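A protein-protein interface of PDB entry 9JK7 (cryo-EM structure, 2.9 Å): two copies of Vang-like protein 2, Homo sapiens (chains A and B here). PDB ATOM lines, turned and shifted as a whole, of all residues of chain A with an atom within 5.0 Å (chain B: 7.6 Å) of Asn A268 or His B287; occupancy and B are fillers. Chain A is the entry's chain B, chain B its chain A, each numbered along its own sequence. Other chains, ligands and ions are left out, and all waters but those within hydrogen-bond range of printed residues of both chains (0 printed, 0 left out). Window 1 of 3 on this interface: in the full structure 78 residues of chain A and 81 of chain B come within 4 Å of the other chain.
Among the printed residues, merely in contact across the chains: Pro A250 with Glu B283, Phe A266 with Pro B452, Phe A266 with His B287, Phe A266 with Ile B454, Thr A253 with Ile B454, Thr A253 with His B287, Phe A266 with Gln B455 and Val A500 with Glu B283.
The backbone carbonyl oxygen of Tyr B286 is in hydrogen-bond range of the backbone NH of Ile B454, at 2.8 Å. OD1 of Asp B288 sits close to ND1 of His B287, at 3.3 Å. OD1 of Asn A268 lies close to O of Phe A252. The side-chain hydroxyl (OG1) of Thr A253 is in hydrogen-bond range of the side-chain amide oxygen (OD1) of Asn A268 (2.7 Å).
Printed residues of chain A that touch a printed residue of chain B: Pro A250, Thr A253, Phe A266, Asn A268 and Val A500. Hydrophobic or aromatic side chains of chain A that line the printed part of chain B: Pro A250, Phe A266 and Val A500. Among the printed residues, no Asp or Glu carboxylate lies within 4 Å of a Lys or Arg side-chain nitrogen of the other chain.
2 positions are printed for both chains.
The backbone carbonyl oxygen (O) of Glu B283 lies within hydrogen-bond range of the side-chain amide nitrogen (ND2) of Asn A268, 3.1 Å away. NE2 of His B287 lies within hydrogen-bond range of ND2 of Asn A268 (2.9 Å).
Asn A268 touches just these residues of chain B: Glu B283 and His B287. Printed residues of chain A within 4 Å of Glu B283: Pro A250, Asn A268 and Val A500. Tyr B286 touches none of the printed residues of chain A. Printed residues of chain A within 4 Å of His B287: Thr A253 (3.7 Å), Phe A266 (3.4 Å) and Asn A268 (2.9 Å). Pro B290 touches none of the printed residues of chain A. Of the printed residues of chain A, Ile B454 touches Thr A253 and Phe A266. Of the printed residues of chain A, Gln B455 touches Phe A266. The nearest residue of chain B that does not touch Asn A268 is Lys B284 (4.2 Å). The nearest printed residue of chain A that does not touch Glu B283 is Thr A253 (5.0 Å).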
ATOM      1  N   PRO A 250      17.794  -8.277 -18.574  1.00  0.00           N
ATOM      2  CA  PRO A 250      17.570  -7.995 -17.150  1.00  0.00           C
ATOM      3  C   PRO A 250      17.392  -6.506 -16.909  1.00  0.00           C
ATOM      4  O   PRO A 250      18.318  -5.715 -17.101  1.00  0.00           O
ATOM      5  CB  PRO A 250      18.839  -8.533 -16.483  1.00  0.00           C
ATOM      6  CG  PRO A 250      19.866  -8.473 -17.539  1.00  0.00           C
ATOM      7  CD  PRO A 250      19.165  -8.745 -18.835  1.00  0.00           C
ATOM      8  N   PHE A 252      15.604  -5.356 -13.861  1.00  0.00           N
ATOM      9  CA  PHE A 252      15.440  -5.101 -12.440  1.00  0.00           C
ATOM     10  C   PHE A 252      16.225  -6.127 -11.641  1.00  0.00           C
ATOM     11  O   PHE A 252      16.483  -7.236 -12.112  1.00  0.00           O
ATOM     12  CB  PHE A 252      13.965  -5.159 -12.030  1.00  0.00           C
ATOM     13  CG  PHE A 252      13.114  -4.142 -12.717  1.00  0.00           C
ATOM     14  CD1 PHE A 252      13.079  -2.836 -12.273  1.00  0.00           C
ATOM     15  CD2 PHE A 252      12.360  -4.489 -13.819  1.00  0.00           C
ATOM     16  CE1 PHE A 252      12.305  -1.900 -12.912  1.00  0.00           C
ATOM     17  CE2 PHE A 252      11.583  -3.558 -14.459  1.00  0.00           C
ATOM     18  CZ  PHE A 252      11.555  -2.261 -14.006  1.00  0.00           C
ATOM     19  N   THR A 253      16.594  -5.745 -10.423  1.00  0.00           N
ATOM     20  CA  THR A 253      17.230  -6.627  -9.461  1.00  0.00           C
ATOM     21  C   THR A 253      16.313  -6.768  -8.258  1.00  0.00           C
ATOM     22  O   THR A 253      15.865  -5.769  -7.684  1.00  0.00           O
ATOM     23  CB  THR A 253      18.595  -6.093  -9.028  1.00  0.00           C
ATOM     24  OG1 THR A 253      19.459  -5.999 -10.165  1.00  0.00           O
ATOM     25  CG2 THR A 253      19.227  -7.014  -8.001  1.00  0.00           C
ATOM     26  N   PHE A 266      19.694 -12.145  -4.508  1.00  0.00           N
ATOM     27  CA  PHE A 266      19.355 -11.113  -5.476  1.00  0.00           C
ATOM     28  C   PHE A 266      19.295 -11.748  -6.854  1.00  0.00           C
ATOM     29  O   PHE A 266      20.093 -12.635  -7.173  1.00  0.00           O
ATOM     30  CB  PHE A 266      20.344  -9.943  -5.508  1.00  0.00           C
ATOM     31  CG  PHE A 266      20.455  -9.166  -4.225  1.00  0.00           C
ATOM     32  CD1 PHE A 266      20.011  -9.675  -3.021  1.00  0.00           C
ATOM     33  CD2 PHE A 266      20.881  -7.852  -4.263  1.00  0.00           C
ATOM     34  CE1 PHE A 266      20.116  -8.943  -1.871  1.00  0.00           C
ATOM     35  CE2 PHE A 266      20.945  -7.102  -3.120  1.00  0.00           C
ATOM     36  CZ  PHE A 266      20.566  -7.647  -1.919  1.00  0.00           C
ATOM     37  N   TYR A 267      18.347 -11.292  -7.661  1.00  0.00           N
ATOM     38  CA  TYR A 267      18.123 -11.843  -8.986  1.00  0.00           C
ATOM     39  C   TYR A 267      17.982 -10.709  -9.987  1.00  0.00           C
ATOM     40  O   TYR A 267      17.627  -9.591  -9.623  1.00  0.00           O
ATOM     41  CB  TYR A 267      16.869 -12.704  -9.021  1.00  0.00           C
ATOM     42  CG  TYR A 267      16.905 -13.878  -8.081  1.00  0.00           C
ATOM     43  CD1 TYR A 267      17.677 -14.992  -8.360  1.00  0.00           C
ATOM     44  CD2 TYR A 267      16.140 -13.883  -6.927  1.00  0.00           C
ATOM     45  CE1 TYR A 267      17.706 -16.067  -7.503  1.00  0.00           C
ATOM     46  CE2 TYR A 267      16.159 -14.954  -6.068  1.00  0.00           C
ATOM     47  CZ  TYR A 267      16.942 -16.041  -6.361  1.00  0.00           C
ATOM     48  OH  TYR A 267      16.957 -17.106  -5.499  1.00  0.00           O
ATOM     49  N   ASN A 268      18.263 -10.997 -11.252  1.00  0.00           N
ATOM     50  CA  ASN A 268      17.951 -10.078 -12.337  1.00  0.00           C
ATOM     51  C   ASN A 268      16.765 -10.620 -13.120  1.00  0.00           C
ATOM     52  O   ASN A 268      16.737 -11.799 -13.481  1.00  0.00           O
ATOM     53  CB  ASN A 268      19.140  -9.858 -13.267  1.00  0.00           C
ATOM     54  CG  ASN A 268      20.134  -8.865 -12.720  1.00  0.00           C
ATOM     55  OD1 ASN A 268      19.759  -7.878 -12.089  1.00  0.00           O
ATOM     56  ND2 ASN A 268      21.407  -9.090 -13.002  1.00  0.00           N
ATOM     57  N   VAL A 269      15.798  -9.752 -13.385  1.00  0.00           N
ATOM     58  CA  VAL A 269      14.576 -10.129 -14.073  1.00  0.00           C
ATOM     59  C   VAL A 269      14.215  -9.030 -15.064  1.00  0.00           C
ATOM     60  O   VAL A 269      14.466  -7.845 -14.827  1.00  0.00           O
ATOM     61  CB  VAL A 269      13.431 -10.389 -13.068  1.00  0.00           C
ATOM     62  CG1 VAL A 269      13.059  -9.114 -12.348  1.00  0.00           C
ATOM     63  CG2 VAL A 269      12.227 -11.001 -13.755  1.00  0.00           C
ATOM     64  N   GLY A 270      13.657  -9.435 -16.197  1.00  0.00           N
ATOM     65  CA  GLY A 270      13.201  -8.510 -17.210  1.00  0.00           C
ATOM     66  C   GLY A 270      11.812  -7.988 -16.915  1.00  0.00           C
ATOM     67  O   GLY A 270      11.313  -8.066 -15.790  1.00  0.00           O
ATOM     68  N   TRP A 280       8.178 -16.725 -10.975  1.00  0.00           N
ATOM     69  CA  TRP A 280       9.603 -16.859 -11.258  1.00  0.00           C
ATOM     70  C   TRP A 280      10.407 -17.006  -9.969  1.00  0.00           C
ATOM     71  O   TRP A 280      11.266 -17.893  -9.848  1.00  0.00           O
ATOM     72  CB  TRP A 280      10.051 -15.635 -12.053  1.00  0.00           C
ATOM     73  CG  TRP A 280      11.443 -15.653 -12.541  1.00  0.00           C
ATOM     74  CD1 TRP A 280      11.955 -16.429 -13.532  1.00  0.00           C
ATOM     75  CD2 TRP A 280      12.521 -14.850 -12.061  1.00  0.00           C
ATOM     76  NE1 TRP A 280      13.288 -16.157 -13.704  1.00  0.00           N
ATOM     77  CE2 TRP A 280      13.659 -15.190 -12.809  1.00  0.00           C
ATOM     78  CE3 TRP A 280      12.632 -13.874 -11.067  1.00  0.00           C
ATOM     79  CZ2 TRP A 280      14.891 -14.593 -12.598  1.00  0.00           C
ATOM     80  CZ3 TRP A 280      13.855 -13.284 -10.860  1.00  0.00           C
ATOM     81  CH2 TRP A 280      14.968 -13.643 -11.622  1.00  0.00           C
ATOM     82  N   VAL A 500      17.952  -1.930 -12.368  1.00  0.00           N
ATOM     83  CA  VAL A 500      19.386  -2.012 -12.667  1.00  0.00           C
ATOM     84  C   VAL A 500      19.842  -0.676 -13.238  1.00  0.00           C
ATOM     85  O   VAL A 500      19.252  -0.189 -14.222  1.00  0.00           O
ATOM     86  CB  VAL A 500      19.670  -3.159 -13.650  1.00  0.00           C
ATOM     87  CG1 VAL A 500      21.131  -3.176 -14.039  1.00  0.00           C
ATOM     88  CG2 VAL A 500      19.282  -4.485 -13.040  1.00  0.00           C
ATOM     89  N   ARG B 265      33.684 -14.228  -9.254  1.00  0.00           N
ATOM     90  CA  ARG B 265      32.592 -15.058  -9.746  1.00  0.00           C
ATOM     91  C   ARG B 265      32.880 -15.466 -11.179  1.00  0.00           C
ATOM     92  O   ARG B 265      33.440 -14.686 -11.952  1.00  0.00           O
ATOM     93  CB  ARG B 265      31.234 -14.344  -9.698  1.00  0.00           C
ATOM     94  CG  ARG B 265      30.738 -13.942  -8.324  1.00  0.00           C
ATOM     95  CD  ARG B 265      30.444 -15.103  -7.410  1.00  0.00           C
ATOM     96  NE  ARG B 265      29.792 -14.634  -6.191  1.00  0.00           N
ATOM     97  CZ  ARG B 265      30.438 -14.164  -5.130  1.00  0.00           C
ATOM     98  NH1 ARG B 265      31.760 -14.082  -5.136  1.00  0.00           N
ATOM     99  NH2 ARG B 265      29.759 -13.762  -4.064  1.00  0.00           N
ATOM    100  N   TYR B 267      31.173 -16.781 -14.811  1.00  0.00           N
ATOM    101  CA  TYR B 267      29.916 -16.672 -15.531  1.00  0.00           C
ATOM    102  C   TYR B 267      30.046 -17.353 -16.881  1.00  0.00           C
ATOM    103  O   TYR B 267      31.145 -17.496 -17.409  1.00  0.00           O
ATOM    104  CB  TYR B 267      29.523 -15.216 -15.738  1.00  0.00           C
ATOM    105  CG  TYR B 267      29.344 -14.442 -14.460  1.00  0.00           C
ATOM    106  CD1 TYR B 267      28.227 -14.630 -13.663  1.00  0.00           C
ATOM    107  CD2 TYR B 267      30.277 -13.499 -14.066  1.00  0.00           C
ATOM    108  CE1 TYR B 267      28.059 -13.919 -12.499  1.00  0.00           C
ATOM    109  CE2 TYR B 267      30.117 -12.782 -12.908  1.00  0.00           C
ATOM    110  CZ  TYR B 267      29.007 -12.994 -12.129  1.00  0.00           C
ATOM    111  OH  TYR B 267      28.853 -12.275 -10.974  1.00  0.00           O
ATOM    112  N   TRP B 280      26.985  -6.502 -19.363  1.00  0.00           N
ATOM    113  CA  TRP B 280      26.431  -7.706 -18.756  1.00  0.00           C
ATOM    114  C   TRP B 280      27.065  -7.979 -17.395  1.00  0.00           C
ATOM    115  O   TRP B 280      26.367  -8.244 -16.405  1.00  0.00           O
ATOM    116  CB  TRP B 280      26.655  -8.873 -19.714  1.00  0.00           C
ATOM    117  CG  TRP B 280      26.047 -10.159 -19.324  1.00  0.00           C
ATOM    118  CD1 TRP B 280      24.723 -10.474 -19.322  1.00  0.00           C
ATOM    119  CD2 TRP B 280      26.738 -11.324 -18.876  1.00  0.00           C
ATOM    120  NE1 TRP B 280      24.547 -11.766 -18.903  1.00  0.00           N
ATOM    121  CE2 TRP B 280      25.771 -12.310 -18.621  1.00  0.00           C
ATOM    122  CE3 TRP B 280      28.085 -11.628 -18.664  1.00  0.00           C
ATOM    123  CZ2 TRP B 280      26.105 -13.575 -18.166  1.00  0.00           C
ATOM    124  CZ3 TRP B 280      28.412 -12.883 -18.213  1.00  0.00           C
ATOM    125  CH2 TRP B 280      27.428 -13.842 -17.969  1.00  0.00           C
ATOM    126  N   ILE B 281      28.393  -7.891 -17.325  1.00  0.00           N
ATOM    127  CA  ILE B 281      29.102  -8.131 -16.074  1.00  0.00           C
ATOM    128  C   ILE B 281      28.767  -7.056 -15.052  1.00  0.00           C
ATOM    129  O   ILE B 281      28.733  -7.322 -13.850  1.00  0.00           O
ATOM    130  CB  ILE B 281      30.616  -8.217 -16.334  1.00  0.00           C
ATOM    131  CG1 ILE B 281      30.930  -9.421 -17.211  1.00  0.00           C
ATOM    132  CG2 ILE B 281      31.387  -8.318 -15.034  1.00  0.00           C
ATOM    133  CD1 ILE B 281      32.318  -9.404 -17.754  1.00  0.00           C
ATOM    134  N   LEU B 282      28.500  -5.831 -15.504  1.00  0.00           N
ATOM    135  CA  LEU B 282      28.107  -4.789 -14.560  1.00  0.00           C
ATOM    136  C   LEU B 282      26.718  -5.055 -13.999  1.00  0.00           C
ATOM    137  O   LEU B 282      26.475  -4.866 -12.803  1.00  0.00           O
ATOM    138  CB  LEU B 282      28.156  -3.419 -15.226  1.00  0.00           C
ATOM    139  CG  LEU B 282      29.555  -2.989 -15.634  1.00  0.00           C
ATOM    140  CD1 LEU B 282      29.528  -1.629 -16.297  1.00  0.00           C
ATOM    141  CD2 LEU B 282      30.457  -3.014 -14.430  1.00  0.00           C
ATOM    142  N   GLU B 283      25.794  -5.492 -14.854  1.00  0.00           N
ATOM    143  CA  GLU B 283      24.472  -5.888 -14.384  1.00  0.00           C
ATOM    144  C   GLU B 283      24.570  -7.026 -13.380  1.00  0.00           C
ATOM    145  O   GLU B 283      23.740  -7.137 -12.472  1.00  0.00           O
ATOM    146  CB  GLU B 283      23.605  -6.290 -15.574  1.00  0.00           C
ATOM    147  CG  GLU B 283      23.296  -5.141 -16.509  1.00  0.00           C
ATOM    148  CD  GLU B 283      22.585  -5.584 -17.765  1.00  0.00           C
ATOM    149  OE1 GLU B 283      22.452  -6.806 -17.969  1.00  0.00           O
ATOM    150  OE2 GLU B 283      22.169  -4.713 -18.556  1.00  0.00           O
ATOM    151  N   LYS B 284      25.575  -7.891 -13.534  1.00  0.00           N
ATOM    152  CA  LYS B 284      25.775  -8.961 -12.559  1.00  0.00           C
ATOM    153  C   LYS B 284      26.462  -8.468 -11.288  1.00  0.00           C
ATOM    154  O   LYS B 284      26.213  -9.007 -10.203  1.00  0.00           O
ATOM    155  CB  LYS B 284      26.589 -10.096 -13.177  1.00  0.00           C
ATOM    156  CG  LYS B 284      25.889 -10.837 -14.293  1.00  0.00           C
ATOM    157  CD  LYS B 284      24.719 -11.627 -13.745  1.00  0.00           C
ATOM    158  CE  LYS B 284      24.020 -12.420 -14.830  1.00  0.00           C
ATOM    159  NZ  LYS B 284      24.855 -13.553 -15.308  1.00  0.00           N
ATOM    160  N   TYR B 285      27.329  -7.463 -11.405  1.00  0.00           N
ATOM    161  CA  TYR B 285      28.167  -7.056 -10.283  1.00  0.00           C
ATOM    162  C   TYR B 285      27.349  -6.493  -9.132  1.00  0.00           C
ATOM    163  O   TYR B 285      27.600  -6.825  -7.969  1.00  0.00           O
ATOM    164  CB  TYR B 285      29.203  -6.031 -10.749  1.00  0.00           C
ATOM    165  CG  TYR B 285      29.977  -5.420  -9.607  1.00  0.00           C
ATOM    166  CD1 TYR B 285      30.924  -6.150  -8.917  1.00  0.00           C
ATOM    167  CD2 TYR B 285      29.753  -4.110  -9.219  1.00  0.00           C
ATOM    168  CE1 TYR B 285      31.621  -5.597  -7.870  1.00  0.00           C
ATOM    169  CE2 TYR B 285      30.445  -3.548  -8.171  1.00  0.00           C
ATOM    170  CZ  TYR B 285      31.380  -4.301  -7.499  1.00  0.00           C
ATOM    171  OH  TYR B 285      32.082  -3.762  -6.451  1.00  0.00           O
ATOM    172  N   TYR B 286      26.366  -5.647  -9.429  1.00  0.00           N
ATOM    173  CA  TYR B 286      25.655  -4.950  -8.367  1.00  0.00           C
ATOM    174  C   TYR B 286      24.802  -5.868  -7.506  1.00  0.00           C
ATOM    175  O   TYR B 286      24.242  -5.398  -6.514  1.00  0.00           O
ATOM    176  CB  TYR B 286      24.800  -3.833  -8.959  1.00  0.00           C
ATOM    177  CG  TYR B 286      25.619  -2.640  -9.378  1.00  0.00           C
ATOM    178  CD1 TYR B 286      26.914  -2.482  -8.928  1.00  0.00           C
ATOM    179  CD2 TYR B 286      25.102  -1.673 -10.212  1.00  0.00           C
ATOM    180  CE1 TYR B 286      27.675  -1.400  -9.300  1.00  0.00           C
ATOM    181  CE2 TYR B 286      25.854  -0.582 -10.585  1.00  0.00           C
ATOM    182  CZ  TYR B 286      27.139  -0.454 -10.131  1.00  0.00           C
ATOM    183  OH  TYR B 286      27.891   0.631 -10.506  1.00  0.00           O
ATOM    184  N   HIS B 287      24.703  -7.154  -7.831  1.00  0.00           N
ATOM    185  CA  HIS B 287      24.022  -8.084  -6.949  1.00  0.00           C
ATOM    186  C   HIS B 287      24.806  -9.365  -6.695  1.00  0.00           C
ATOM    187  O   HIS B 287      24.351 -10.194  -5.902  1.00  0.00           O
ATOM    188  CB  HIS B 287      22.638  -8.444  -7.504  1.00  0.00           C
ATOM    189  CG  HIS B 287      22.677  -9.344  -8.695  1.00  0.00           C
ATOM    190  ND1 HIS B 287      22.690 -10.717  -8.585  1.00  0.00           N
ATOM    191  CD2 HIS B 287      22.708  -9.073 -10.020  1.00  0.00           C
ATOM    192  CE1 HIS B 287      22.726 -11.253  -9.790  1.00  0.00           C
ATOM    193  NE2 HIS B 287      22.741 -10.277 -10.678  1.00  0.00           N
ATOM    194  N   ASP B 288      25.960  -9.559  -7.338  1.00  0.00           N
ATOM    195  CA  ASP B 288      26.767 -10.754  -7.107  1.00  0.00           C
ATOM    196  C   ASP B 288      27.899 -10.518  -6.112  1.00  0.00           C
ATOM    197  O   ASP B 288      27.989 -11.222  -5.104  1.00  0.00           O
ATOM    198  CB  ASP B 288      27.328 -11.287  -8.428  1.00  0.00           C
ATOM    199  CG  ASP B 288      26.289 -12.020  -9.244  1.00  0.00           C
ATOM    200  OD1 ASP B 288      25.354 -12.586  -8.643  1.00  0.00           O
ATOM    201  OD2 ASP B 288      26.410 -12.041 -10.486  1.00  0.00           O
ATOM    202  N   PHE B 289      28.772  -9.549  -6.373  1.00  0.00           N
ATOM    203  CA  PHE B 289      29.871  -9.333  -5.449  1.00  0.00           C
ATOM    204  C   PHE B 289      29.370  -8.574  -4.226  1.00  0.00           C
ATOM    205  O   PHE B 289      28.406  -7.810  -4.312  1.00  0.00           O
ATOM    206  CB  PHE B 289      31.013  -8.529  -6.071  1.00  0.00           C
ATOM    207  CG  PHE B 289      31.713  -9.201  -7.214  1.00  0.00           C
ATOM    208  CD1 PHE B 289      31.299 -10.414  -7.712  1.00  0.00           C
ATOM    209  CD2 PHE B 289      32.863  -8.643  -7.728  1.00  0.00           C
ATOM    210  CE1 PHE B 289      31.970 -11.001  -8.754  1.00  0.00           C
ATOM    211  CE2 PHE B 289      33.537  -9.240  -8.755  1.00  0.00           C
ATOM    212  CZ  PHE B 289      33.092 -10.421  -9.266  1.00  0.00           C
ATOM    213  N   PRO B 290      30.011  -8.760  -3.076  1.00  0.00           N
ATOM    214  CA  PRO B 290      29.740  -7.876  -1.941  1.00  0.00           C
ATOM    215  C   PRO B 290      30.108  -6.444  -2.286  1.00  0.00           C
ATOM    216  O   PRO B 290      30.908  -6.185  -3.187  1.00  0.00           O
ATOM    217  CB  PRO B 290      30.642  -8.429  -0.833  1.00  0.00           C
ATOM    218  CG  PRO B 290      30.895  -9.844  -1.227  1.00  0.00           C
ATOM    219  CD  PRO B 290      30.954  -9.833  -2.723  1.00  0.00           C
ATOM    220  N   GLY B 451      26.904  -7.900   1.933  1.00  0.00           N
ATOM    221  CA  GLY B 451      25.833  -7.583   1.020  1.00  0.00           C
ATOM    222  C   GLY B 451      26.320  -6.907  -0.245  1.00  0.00           C
ATOM    223  O   GLY B 451      27.336  -6.206  -0.253  1.00  0.00           O
ATOM    224  N   PRO B 452      25.600  -7.104  -1.341  1.00  0.00           N
ATOM    225  CA  PRO B 452      26.036  -6.562  -2.629  1.00  0.00           C
ATOM    226  C   PRO B 452      25.710  -5.082  -2.776  1.00  0.00           C
ATOM    227  O   PRO B 452      25.069  -4.460  -1.931  1.00  0.00           O
ATOM    228  CB  PRO B 452      25.262  -7.405  -3.642  1.00  0.00           C
ATOM    229  CG  PRO B 452      24.074  -7.842  -2.922  1.00  0.00           C
ATOM    230  CD  PRO B 452      24.464  -8.024  -1.491  1.00  0.00           C
ATOM    231  N   THR B 453      26.165  -4.529  -3.903  1.00  0.00           N
ATOM    232  CA  THR B 453      26.199  -3.082  -4.076  1.00  0.00           C
ATOM    233  C   THR B 453      24.801  -2.489  -4.193  1.00  0.00           C
ATOM    234  O   THR B 453      24.537  -1.408  -3.657  1.00  0.00           O
ATOM    235  CB  THR B 453      27.025  -2.730  -5.309  1.00  0.00           C
ATOM    236  OG1 THR B 453      28.344  -3.266  -5.166  1.00  0.00           O
ATOM    237  CG2 THR B 453      27.116  -1.226  -5.478  1.00  0.00           C
ATOM    238  N   ILE B 454      23.892  -3.171  -4.893  1.00  0.00           N
ATOM    239  CA  ILE B 454      22.582  -2.586  -5.145  1.00  0.00           C
ATOM    240  C   ILE B 454      21.765  -2.507  -3.868  1.00  0.00           C
ATOM    241  O   ILE B 454      20.806  -1.733  -3.791  1.00  0.00           O
ATOM    242  CB  ILE B 454      21.839  -3.378  -6.236  1.00  0.00           C
ATOM    243  CG1 ILE B 454      20.704  -2.546  -6.821  1.00  0.00           C
ATOM    244  CG2 ILE B 454      21.275  -4.662  -5.669  1.00  0.00           C
ATOM    245  CD1 ILE B 454      20.181  -3.074  -8.119  1.00  0.00           C
ATOM    246  N   GLN B 455      22.142  -3.275  -2.847  1.00  0.00           N
ATOM    247  CA  GLN B 455      21.455  -3.254  -1.564  1.00  0.00           C
ATOM    248  C   GLN B 455      21.558  -1.903  -0.867  1.00  0.00           C
ATOM    249  O   GLN B 455      20.728  -1.599  -0.006  1.00  0.00           O
ATOM    250  CB  GLN B 455      22.040  -4.354  -0.681  1.00  0.00           C
ATOM    251  CG  GLN B 455      21.349  -4.595   0.634  1.00  0.00           C
ATOM    252  CD  GLN B 455      21.977  -5.741   1.387  1.00  0.00           C
ATOM    253  OE1 GLN B 455      22.984  -6.292   0.961  1.00  0.00           O
ATOM    254  NE2 GLN B 455      21.375  -6.122   2.500  1.00  0.00           N
